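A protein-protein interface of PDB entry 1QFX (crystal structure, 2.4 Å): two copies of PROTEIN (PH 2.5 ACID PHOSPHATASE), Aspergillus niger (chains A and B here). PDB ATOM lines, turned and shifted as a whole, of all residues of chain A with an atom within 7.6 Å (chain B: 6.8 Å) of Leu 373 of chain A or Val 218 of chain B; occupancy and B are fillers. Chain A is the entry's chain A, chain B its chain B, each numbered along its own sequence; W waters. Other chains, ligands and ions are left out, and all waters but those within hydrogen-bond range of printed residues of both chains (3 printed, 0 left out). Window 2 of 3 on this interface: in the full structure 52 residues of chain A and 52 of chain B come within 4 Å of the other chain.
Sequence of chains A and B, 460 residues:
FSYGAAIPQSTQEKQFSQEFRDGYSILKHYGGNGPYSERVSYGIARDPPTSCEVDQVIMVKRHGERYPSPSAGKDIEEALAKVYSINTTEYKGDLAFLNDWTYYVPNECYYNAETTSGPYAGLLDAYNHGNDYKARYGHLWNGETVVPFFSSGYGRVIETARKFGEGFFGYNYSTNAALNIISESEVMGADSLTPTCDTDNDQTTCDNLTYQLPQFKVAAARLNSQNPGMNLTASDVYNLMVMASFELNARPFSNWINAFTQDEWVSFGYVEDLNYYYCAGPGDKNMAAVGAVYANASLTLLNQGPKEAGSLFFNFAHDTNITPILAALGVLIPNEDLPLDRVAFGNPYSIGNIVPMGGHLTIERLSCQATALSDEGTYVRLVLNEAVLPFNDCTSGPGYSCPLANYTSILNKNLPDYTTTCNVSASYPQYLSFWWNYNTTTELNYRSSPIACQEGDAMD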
ATOM      1  N   THR A  50       2.495  -2.006  31.742  1.00  0.00           N
ATOM      2  CA  THR A  50       1.156  -1.957  32.324  1.00  0.00           C
ATOM      3  C   THR A  50       0.834  -3.406  32.722  1.00  0.00           C
ATOM      4  O   THR A  50       1.226  -4.333  31.990  1.00  0.00           O
ATOM      5  CB  THR A  50       0.166  -1.454  31.283  1.00  0.00           C
ATOM      6  OG1 THR A  50       0.362  -0.050  31.124  1.00  0.00           O
ATOM      7  CG2 THR A  50      -1.270  -1.708  31.707  1.00  0.00           C
ATOM      8  N   SER A  51       0.193  -3.589  33.887  1.00  0.00           N
ATOM      9  CA  SER A  51      -0.151  -4.910  34.438  1.00  0.00           C
ATOM     10  C   SER A  51       0.971  -5.524  35.286  1.00  0.00           C
ATOM     11  O   SER A  51       0.805  -6.632  35.814  1.00  0.00           O
ATOM     12  CB  SER A  51      -0.502  -5.920  33.331  1.00  0.00           C
ATOM     13  OG  SER A  51      -1.657  -5.541  32.595  1.00  0.00           O
ATOM     14  N   ALA A 370      -2.056 -11.017  33.954  1.00  0.00           N
ATOM     15  CA  ALA A 370      -2.106 -11.471  32.563  1.00  0.00           C
ATOM     16  C   ALA A 370      -2.279 -10.290  31.606  1.00  0.00           C
ATOM     17  O   ALA A 370      -2.898  -9.284  31.961  1.00  0.00           O
ATOM     18  CB  ALA A 370      -3.223 -12.459  32.367  1.00  0.00           C
ATOM     19  N   THR A 371      -1.645 -10.371  30.439  1.00  0.00           N
ATOM     20  CA  THR A 371      -1.761  -9.319  29.429  1.00  0.00           C
ATOM     21  C   THR A 371      -2.149 -10.058  28.165  1.00  0.00           C
ATOM     22  O   THR A 371      -2.079 -11.286  28.120  1.00  0.00           O
ATOM     23  CB  THR A 371      -0.426  -8.580  29.171  1.00  0.00           C
ATOM     24  OG1 THR A 371       0.506  -9.469  28.529  1.00  0.00           O
ATOM     25  CG2 THR A 371       0.168  -8.054  30.488  1.00  0.00           C
ATOM     26  N   ALA A 372      -2.493  -9.326  27.119  1.00  0.00           N
ATOM     27  CA  ALA A 372      -2.900  -9.943  25.866  1.00  0.00           C
ATOM     28  C   ALA A 372      -1.807 -10.796  25.250  1.00  0.00           C
ATOM     29  O   ALA A 372      -2.081 -11.533  24.309  1.00  0.00           O
ATOM     30  CB  ALA A 372      -3.337  -8.875  24.893  1.00  0.00           C
ATOM     31  N   LEU A 373      -0.569 -10.689  25.755  1.00  0.00           N
ATOM     32  CA  LEU A 373       0.560 -11.470  25.222  1.00  0.00           C
ATOM     33  C   LEU A 373       1.245 -12.373  26.252  1.00  0.00           C
ATOM     34  O   LEU A 373       2.187 -13.090  25.913  1.00  0.00           O
ATOM     35  CB  LEU A 373       1.601 -10.545  24.574  1.00  0.00           C
ATOM     36  CG  LEU A 373       2.199  -9.359  25.361  1.00  0.00           C
ATOM     37  CD1 LEU A 373       3.153  -9.816  26.493  1.00  0.00           C
ATOM     38  CD2 LEU A 373       2.948  -8.463  24.396  1.00  0.00           C
ATOM     39  N   SER A 374       0.771 -12.371  27.495  1.00  0.00           N
ATOM     40  CA  SER A 374       1.407 -13.196  28.523  1.00  0.00           C
ATOM     41  C   SER A 374       0.503 -13.611  29.691  1.00  0.00           C
ATOM     42  O   SER A 374      -0.480 -12.931  30.044  1.00  0.00           O
ATOM     43  CB  SER A 374       2.612 -12.445  29.097  1.00  0.00           C
ATOM     44  OG  SER A 374       2.200 -11.190  29.643  1.00  0.00           O
ATOM     45  N   ASP A 375       0.897 -14.702  30.329  1.00  0.00           N
ATOM     46  CA  ASP A 375       0.188 -15.214  31.488  1.00  0.00           C
ATOM     47  C   ASP A 375       0.624 -14.440  32.718  1.00  0.00           C
ATOM     48  O   ASP A 375       1.671 -13.764  32.736  1.00  0.00           O
ATOM     49  CB  ASP A 375       0.508 -16.689  31.716  1.00  0.00           C
ATOM     50  CG  ASP A 375      -0.097 -17.581  30.652  1.00  0.00           C
ATOM     51  OD1 ASP A 375      -1.145 -17.182  30.075  1.00  0.00           O
ATOM     52  OD2 ASP A 375       0.480 -18.670  30.387  1.00  0.00           O
ATOM     53  N   TYR A 379       8.381 -12.237  35.918  1.00  0.00           N
ATOM     54  CA  TYR A 379       9.253 -11.982  34.777  1.00  0.00           C
ATOM     55  C   TYR A 379      10.535 -11.306  35.219  1.00  0.00           C
ATOM     56  O   TYR A 379      10.591 -10.692  36.289  1.00  0.00           O
ATOM     57  CB  TYR A 379       8.498 -11.148  33.720  1.00  0.00           C
ATOM     58  CG  TYR A 379       7.318 -11.916  33.137  1.00  0.00           C
ATOM     59  CD1 TYR A 379       7.468 -12.721  32.012  1.00  0.00           C
ATOM     60  CD2 TYR A 379       6.069 -11.874  33.751  1.00  0.00           C
ATOM     61  CE1 TYR A 379       6.407 -13.464  31.515  1.00  0.00           C
ATOM     62  CE2 TYR A 379       4.998 -12.613  33.262  1.00  0.00           C
ATOM     63  CZ  TYR A 379       5.171 -13.405  32.146  1.00  0.00           C
ATOM     64  OH  TYR A 379       4.103 -14.137  31.669  1.00  0.00           O
ATOM     65  N   THR A 395      12.191 -12.842  25.013  1.00  0.00           N
ATOM     66  CA  THR A 395      11.514 -11.561  25.144  1.00  0.00           C
ATOM     67  C   THR A 395       9.992 -11.704  25.025  1.00  0.00           C
ATOM     68  O   THR A 395       9.313 -10.788  24.519  1.00  0.00           O
ATOM     69  CB  THR A 395      12.012 -10.568  24.052  1.00  0.00           C
ATOM     70  OG1 THR A 395      11.818 -11.148  22.754  1.00  0.00           O
ATOM     71  CG2 THR A 395      13.508 -10.260  24.219  1.00  0.00           C
ATOM     72  N   SER A 396       9.460 -12.813  25.546  1.00  0.00           N
ATOM     73  CA  SER A 396       8.030 -13.101  25.494  1.00  0.00           C
ATOM     74  C   SER A 396       7.151 -12.443  26.551  1.00  0.00           C
ATOM     75  O   SER A 396       5.933 -12.361  26.374  1.00  0.00           O
ATOM     76  CB  SER A 396       7.802 -14.600  25.517  1.00  0.00           C
ATOM     77  OG  SER A 396       8.427 -15.187  26.645  1.00  0.00           O
ATOM     78  N   GLY A 397       7.735 -11.968  27.645  1.00  0.00           N
ATOM     79  CA  GLY A 397       6.910 -11.351  28.665  1.00  0.00           C
ATOM     80  C   GLY A 397       6.663  -9.880  28.414  1.00  0.00           C
ATOM     81  O   GLY A 397       7.132  -9.343  27.404  1.00  0.00           O
ATOM     82  N   PRO A 398       5.895  -9.200  29.290  1.00  0.00           N
ATOM     83  CA  PRO A 398       5.606  -7.771  29.137  1.00  0.00           C
ATOM     84  C   PRO A 398       6.920  -6.974  29.044  1.00  0.00           C
ATOM     85  O   PRO A 398       7.897  -7.328  29.691  1.00  0.00           O
ATOM     86  CB  PRO A 398       4.866  -7.450  30.432  1.00  0.00           C
ATOM     87  CG  PRO A 398       4.123  -8.719  30.707  1.00  0.00           C
ATOM     88  CD  PRO A 398       5.156  -9.774  30.431  1.00  0.00           C
ATOM     89  N   GLY A 399       6.934  -5.907  28.250  1.00  0.00           N
ATOM     90  CA  GLY A 399       8.128  -5.092  28.082  1.00  0.00           C
ATOM     91  C   GLY A 399       9.345  -5.869  27.604  1.00  0.00           C
ATOM     92  O   GLY A 399      10.493  -5.538  27.951  1.00  0.00           O
ATOM     93  N   TYR A 400       9.102  -6.901  26.806  1.00  0.00           N
ATOM     94  CA  TYR A 400      10.176  -7.743  26.268  1.00  0.00           C
ATOM     95  C   TYR A 400      10.983  -8.419  27.375  1.00  0.00           C
ATOM     96  O   TYR A 400      12.185  -8.631  27.233  1.00  0.00           O
ATOM     97  CB  TYR A 400      11.106  -6.922  25.348  1.00  0.00           C
ATOM     98  CG  TYR A 400      10.370  -6.215  24.218  1.00  0.00           C
ATOM     99  CD1 TYR A 400      10.040  -6.895  23.042  1.00  0.00           C
ATOM    100  CD2 TYR A 400       9.964  -4.887  24.348  1.00  0.00           C
ATOM    101  CE1 TYR A 400       9.323  -6.275  22.025  1.00  0.00           C
ATOM    102  CE2 TYR A 400       9.247  -4.256  23.346  1.00  0.00           C
ATOM    103  CZ  TYR A 400       8.926  -4.960  22.181  1.00  0.00           C
ATOM    104  OH  TYR A 400       8.184  -4.353  21.184  1.00  0.00           O
ATOM    105  N   SER A 401      10.318  -8.762  28.474  1.00  0.00           N
ATOM    106  CA  SER A 401      10.982  -9.417  29.589  1.00  0.00           C
ATOM    107  C   SER A 401      11.049 -10.917  29.355  1.00  0.00           C
ATOM    108  O   SER A 401      10.547 -11.420  28.346  1.00  0.00           O
ATOM    109  CB  SER A 401      10.282  -9.093  30.914  1.00  0.00           C
ATOM    110  OG  SER A 401       8.905  -9.384  30.839  1.00  0.00           O
ATOM    111  N   LEU B 213       3.094  -9.017  15.489  1.00  0.00           N
ATOM    112  CA  LEU B 213       3.954  -9.327  16.630  1.00  0.00           C
ATOM    113  C   LEU B 213       2.997  -9.176  17.824  1.00  0.00           C
ATOM    114  O   LEU B 213       2.028  -8.401  17.760  1.00  0.00           O
ATOM    115  CB  LEU B 213       5.156  -8.379  16.738  1.00  0.00           C
ATOM    116  CG  LEU B 213       6.418  -8.713  15.931  1.00  0.00           C
ATOM    117  CD1 LEU B 213       7.527  -7.739  16.287  1.00  0.00           C
ATOM    118  CD2 LEU B 213       6.889 -10.125  16.185  1.00  0.00           C
ATOM    119  N   PRO B 214       3.234  -9.930  18.912  1.00  0.00           N
ATOM    120  CA  PRO B 214       2.409  -9.910  20.122  1.00  0.00           C
ATOM    121  C   PRO B 214       1.986  -8.559  20.655  1.00  0.00           C
ATOM    122  O   PRO B 214       0.851  -8.426  21.102  1.00  0.00           O
ATOM    123  CB  PRO B 214       3.267 -10.665  21.137  1.00  0.00           C
ATOM    124  CG  PRO B 214       3.970 -11.664  20.286  1.00  0.00           C
ATOM    125  CD  PRO B 214       4.385 -10.840  19.084  1.00  0.00           C
ATOM    126  N   GLN B 215       2.858  -7.550  20.609  1.00  0.00           N
ATOM    127  CA  GLN B 215       2.477  -6.234  21.143  1.00  0.00           C
ATOM    128  C   GLN B 215       1.221  -5.657  20.514  1.00  0.00           C
ATOM    129  O   GLN B 215       0.508  -4.888  21.160  1.00  0.00           O
ATOM    130  CB  GLN B 215       3.612  -5.215  21.060  1.00  0.00           C
ATOM    131  CG  GLN B 215       4.752  -5.477  22.033  1.00  0.00           C
ATOM    132  CD  GLN B 215       4.465  -5.022  23.453  1.00  0.00           C
ATOM    133  OE1 GLN B 215       5.014  -5.570  24.415  1.00  0.00           O
ATOM    134  NE2 GLN B 215       3.623  -4.018  23.594  1.00  0.00           N
ATOM    135  N   PHE B 216       0.932  -6.040  19.268  1.00  0.00           N
ATOM    136  CA  PHE B 216      -0.264  -5.535  18.585  1.00  0.00           C
ATOM    137  C   PHE B 216      -1.546  -6.024  19.284  1.00  0.00           C
ATOM    138  O   PHE B 216      -2.566  -5.331  19.280  1.00  0.00           O
ATOM    139  CB  PHE B 216      -0.259  -5.913  17.093  1.00  0.00           C
ATOM    140  CG  PHE B 216       0.880  -5.288  16.290  1.00  0.00           C
ATOM    141  CD1 PHE B 216       1.683  -4.273  16.831  1.00  0.00           C
ATOM    142  CD2 PHE B 216       1.174  -5.749  15.001  1.00  0.00           C
ATOM    143  CE1 PHE B 216       2.753  -3.741  16.102  1.00  0.00           C
ATOM    144  CE2 PHE B 216       2.238  -5.222  14.273  1.00  0.00           C
ATOM    145  CZ  PHE B 216       3.030  -4.220  14.823  1.00  0.00           C
ATOM    146  N   LYS B 217      -1.468  -7.197  19.918  1.00  0.00           N
ATOM    147  CA  LYS B 217      -2.586  -7.765  20.677  1.00  0.00           C
ATOM    148  C   LYS B 217      -2.867  -6.897  21.913  1.00  0.00           C
ATOM    149  O   LYS B 217      -4.031  -6.621  22.232  1.00  0.00           O
ATOM    150  CB  LYS B 217      -2.299  -9.213  21.067  1.00  0.00           C
ATOM    151  CG  LYS B 217      -2.361 -10.156  19.876  1.00  0.00           C
ATOM    152  CD  LYS B 217      -2.165 -11.616  20.243  1.00  0.00           C
ATOM    153  CE  LYS B 217      -0.756 -11.886  20.748  1.00  0.00           C
ATOM    154  NZ  LYS B 217      -0.637 -13.160  21.535  1.00  0.00           N
ATOM    155  N   VAL B 218      -1.809  -6.385  22.547  1.00  0.00           N
ATOM    156  CA  VAL B 218      -1.953  -5.528  23.725  1.00  0.00           C
ATOM    157  C   VAL B 218      -2.614  -4.223  23.342  1.00  0.00           C
ATOM    158  O   VAL B 218      -3.463  -3.713  24.078  1.00  0.00           O
ATOM    159  CB  VAL B 218      -0.600  -5.230  24.387  1.00  0.00           C
ATOM    160  CG1 VAL B 218      -0.766  -4.248  25.521  1.00  0.00           C
ATOM    161  CG2 VAL B 218       0.022  -6.510  24.884  1.00  0.00           C
ATOM    162  N   ALA B 219      -2.237  -3.692  22.183  1.00  0.00           N
ATOM    163  CA  ALA B 219      -2.798  -2.430  21.685  1.00  0.00           C
ATOM    164  C   ALA B 219      -4.289  -2.584  21.391  1.00  0.00           C
ATOM    165  O   ALA B 219      -5.108  -1.772  21.844  1.00  0.00           O
ATOM    166  CB  ALA B 219      -2.056  -1.977  20.423  1.00  0.00           C
ATOM    167  N   ALA B 220      -4.625  -3.630  20.633  1.00  0.00           N
ATOM    168  CA  ALA B 220      -6.014  -3.933  20.264  1.00  0.00           C
ATOM    169  C   ALA B 220      -6.875  -4.044  21.525  1.00  0.00           C
ATOM    170  O   ALA B 220      -7.928  -3.403  21.634  1.00  0.00           O
ATOM    171  CB  ALA B 220      -6.069  -5.235  19.473  1.00  0.00           C
ATOM    172  N   ALA B 221      -6.388  -4.817  22.497  1.00  0.00           N
ATOM    173  CA  ALA B 221      -7.084  -5.013  23.762  1.00  0.00           C
ATOM    174  C   ALA B 221      -7.279  -3.703  24.504  1.00  0.00           C
ATOM    175  O   ALA B 221      -8.372  -3.420  25.005  1.00  0.00           O
ATOM    176  CB  ALA B 221      -6.315  -5.995  24.621  1.00  0.00           C
ATOM    177  N   ARG B 222      -6.235  -2.881  24.563  1.00  0.00           N
ATOM    178  CA  ARG B 222      -6.358  -1.604  25.256  1.00  0.00           C
ATOM    179  C   ARG B 222      -7.306  -0.631  24.547  1.00  0.00           C
ATOM    180  O   ARG B 222      -8.095   0.071  25.202  1.00  0.00           O
ATOM    181  CB  ARG B 222      -4.990  -0.954  25.442  1.00  0.00           C
ATOM    182  CG  ARG B 222      -5.029   0.387  26.176  1.00  0.00           C
ATOM    183  CD  ARG B 222      -3.663   1.080  26.183  1.00  0.00           C
ATOM    184  NE  ARG B 222      -3.214   1.391  24.824  1.00  0.00           N
ATOM    185  CZ  ARG B 222      -2.308   0.689  24.147  1.00  0.00           C
ATOM    186  NH1 ARG B 222      -1.691  -0.341  24.709  1.00  0.00           N
ATOM    187  NH2 ARG B 222      -1.981   1.054  22.920  1.00  0.00           N
ATOM    188  N   LEU B 223      -7.230  -0.574  23.220  1.00  0.00           N
ATOM    189  CA  LEU B 223      -8.077   0.342  22.465  1.00  0.00           C
ATOM    190  C   LEU B 223      -9.560  -0.035  22.590  1.00  0.00           C
ATOM    191  O   LEU B 223     -10.403   0.825  22.866  1.00  0.00           O
ATOM    192  CB  LEU B 223      -7.651   0.404  20.987  1.00  0.00           C
ATOM    193  CG  LEU B 223      -6.317   1.038  20.559  1.00  0.00           C
ATOM    194  CD1 LEU B 223      -6.289   1.106  19.052  1.00  0.00           C
ATOM    195  CD2 LEU B 223      -6.171   2.424  21.117  1.00  0.00           C
ATOM    196  N   VAL B 237      -4.771  -2.670  14.241  1.00  0.00           N
ATOM    197  CA  VAL B 237      -3.742  -1.936  14.971  1.00  0.00           C
ATOM    198  C   VAL B 237      -2.548  -1.664  14.054  1.00  0.00           C
ATOM    199  O   VAL B 237      -2.055  -0.541  13.989  1.00  0.00           O
ATOM    200  CB  VAL B 237      -3.316  -2.706  16.240  1.00  0.00           C
ATOM    201  CG1 VAL B 237      -1.988  -2.182  16.782  1.00  0.00           C
ATOM    202  CG2 VAL B 237      -4.415  -2.579  17.287  1.00  0.00           C
ATOM    203  N   THR B 261       1.761   2.490  22.705  1.00  0.00           N
ATOM    204  CA  THR B 261       2.848   2.570  23.650  1.00  0.00           C
ATOM    205  C   THR B 261       4.201   2.537  22.947  1.00  0.00           C
ATOM    206  O   THR B 261       4.311   2.176  21.768  1.00  0.00           O
ATOM    207  CB  THR B 261       2.782   1.396  24.722  1.00  0.00           C
ATOM    208  OG1 THR B 261       2.947   0.127  24.075  1.00  0.00           O
ATOM    209  CG2 THR B 261       1.440   1.407  25.485  1.00  0.00           C
ATOM    210  N   GLU B 264       4.916  -0.819  21.699  1.00  0.00           N
ATOM    211  CA  GLU B 264       4.152  -1.169  20.506  1.00  0.00           C
ATOM    212  C   GLU B 264       4.871  -0.625  19.270  1.00  0.00           C
ATOM    213  O   GLU B 264       5.052  -1.334  18.270  1.00  0.00           O
ATOM    214  CB  GLU B 264       2.723  -0.647  20.633  1.00  0.00           C
ATOM    215  CG  GLU B 264       1.828  -1.635  21.380  1.00  0.00           C
ATOM    216  CD  GLU B 264       0.763  -0.979  22.209  1.00  0.00           C
ATOM    217  OE1 GLU B 264       0.402   0.179  21.941  1.00  0.00           O
ATOM    218  OE2 GLU B 264       0.292  -1.612  23.167  1.00  0.00           O
HETATM  219  O   HOH W   1       1.746 -13.704  22.529  1.00  0.00           O
HETATM  220  O   HOH W   2       4.495  -5.242  27.091  1.00  0.00           O
HETATM  221  O   HOH W   3       6.703  -7.790  25.064  1.00  0.00           O
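Leu 373 of chain A touches just these residues of chain B: Pro 214 (3.8 Å), Gln 215 (3.6 Å) and Val 218 (3.6 Å). Val 218 of chain B touches just these residues of chain A: Ala 372 (3.7 Å) and Leu 373 (3.6 Å). Of the printed residues of chain A, Pro 214 of chain B touches Leu 373 (3.8 Å). Of the printed residues of chain B, Ala 372 of chain A touches Lys 217 (3.5 Å) and Val 218 (3.7 Å). Ala 370 of chain A touches none of the printed residues of chain B. The nearest residue of chain B that does not touch Leu 373 of chain A is Lys 217 of chain B (4.2 Å).
Hydrophobic or aromatic side chains of chain B within 4 Å of the printed part of chain A: Pro 214 and Val 218. Along chain B the printed residues that touch a printed residue of chain A span positions 214 to 218. Of the 16 printed residues of chain A, 3 touch a printed residue of chain B. Along chain A the printed residues that touch a printed residue of chain B span positions 372 to 400.
Water W1 lies within hydrogen-bond range of the side-chain amino group of Lys 217 of chain B and the backbone carbonyl oxygen of Leu 373 of chain A. Water W2 bridges OE1 of Gln 215 of chain B and N of Gly 399 of chain A. Water W3 lies within hydrogen-bond range of O of Gly 397 of chain A, OE1 of Gln 215 of chain B and N of Tyr 400 of chain A.
OG1 of Thr 371 of chain A sits close to N of Leu 373 of chain A, 3.2 Å away.
No position is printed for both chains. Of the 6 pairs that touch across the chains among the printed residues, none has its exchanged pair printed and touching as well.
O of Ala 372 of chain A touches NZ of Lys 217 of chain B, 3.5 Å away. Val 218 of chain B touches Ala 372 of chain A. CB of Pro 214 of chain B touches CB of Leu 373 of chain A, 3.8 Å away. Leu 373 of chain A touches Gln 215 of chain B (CD2 to OE1, 3.6 Å). Leu 373 of chain A touches Val 218 of chain B. Gln 215 of chain B touches Tyr 400 of chain A (CG to OH, 3.7 Å).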
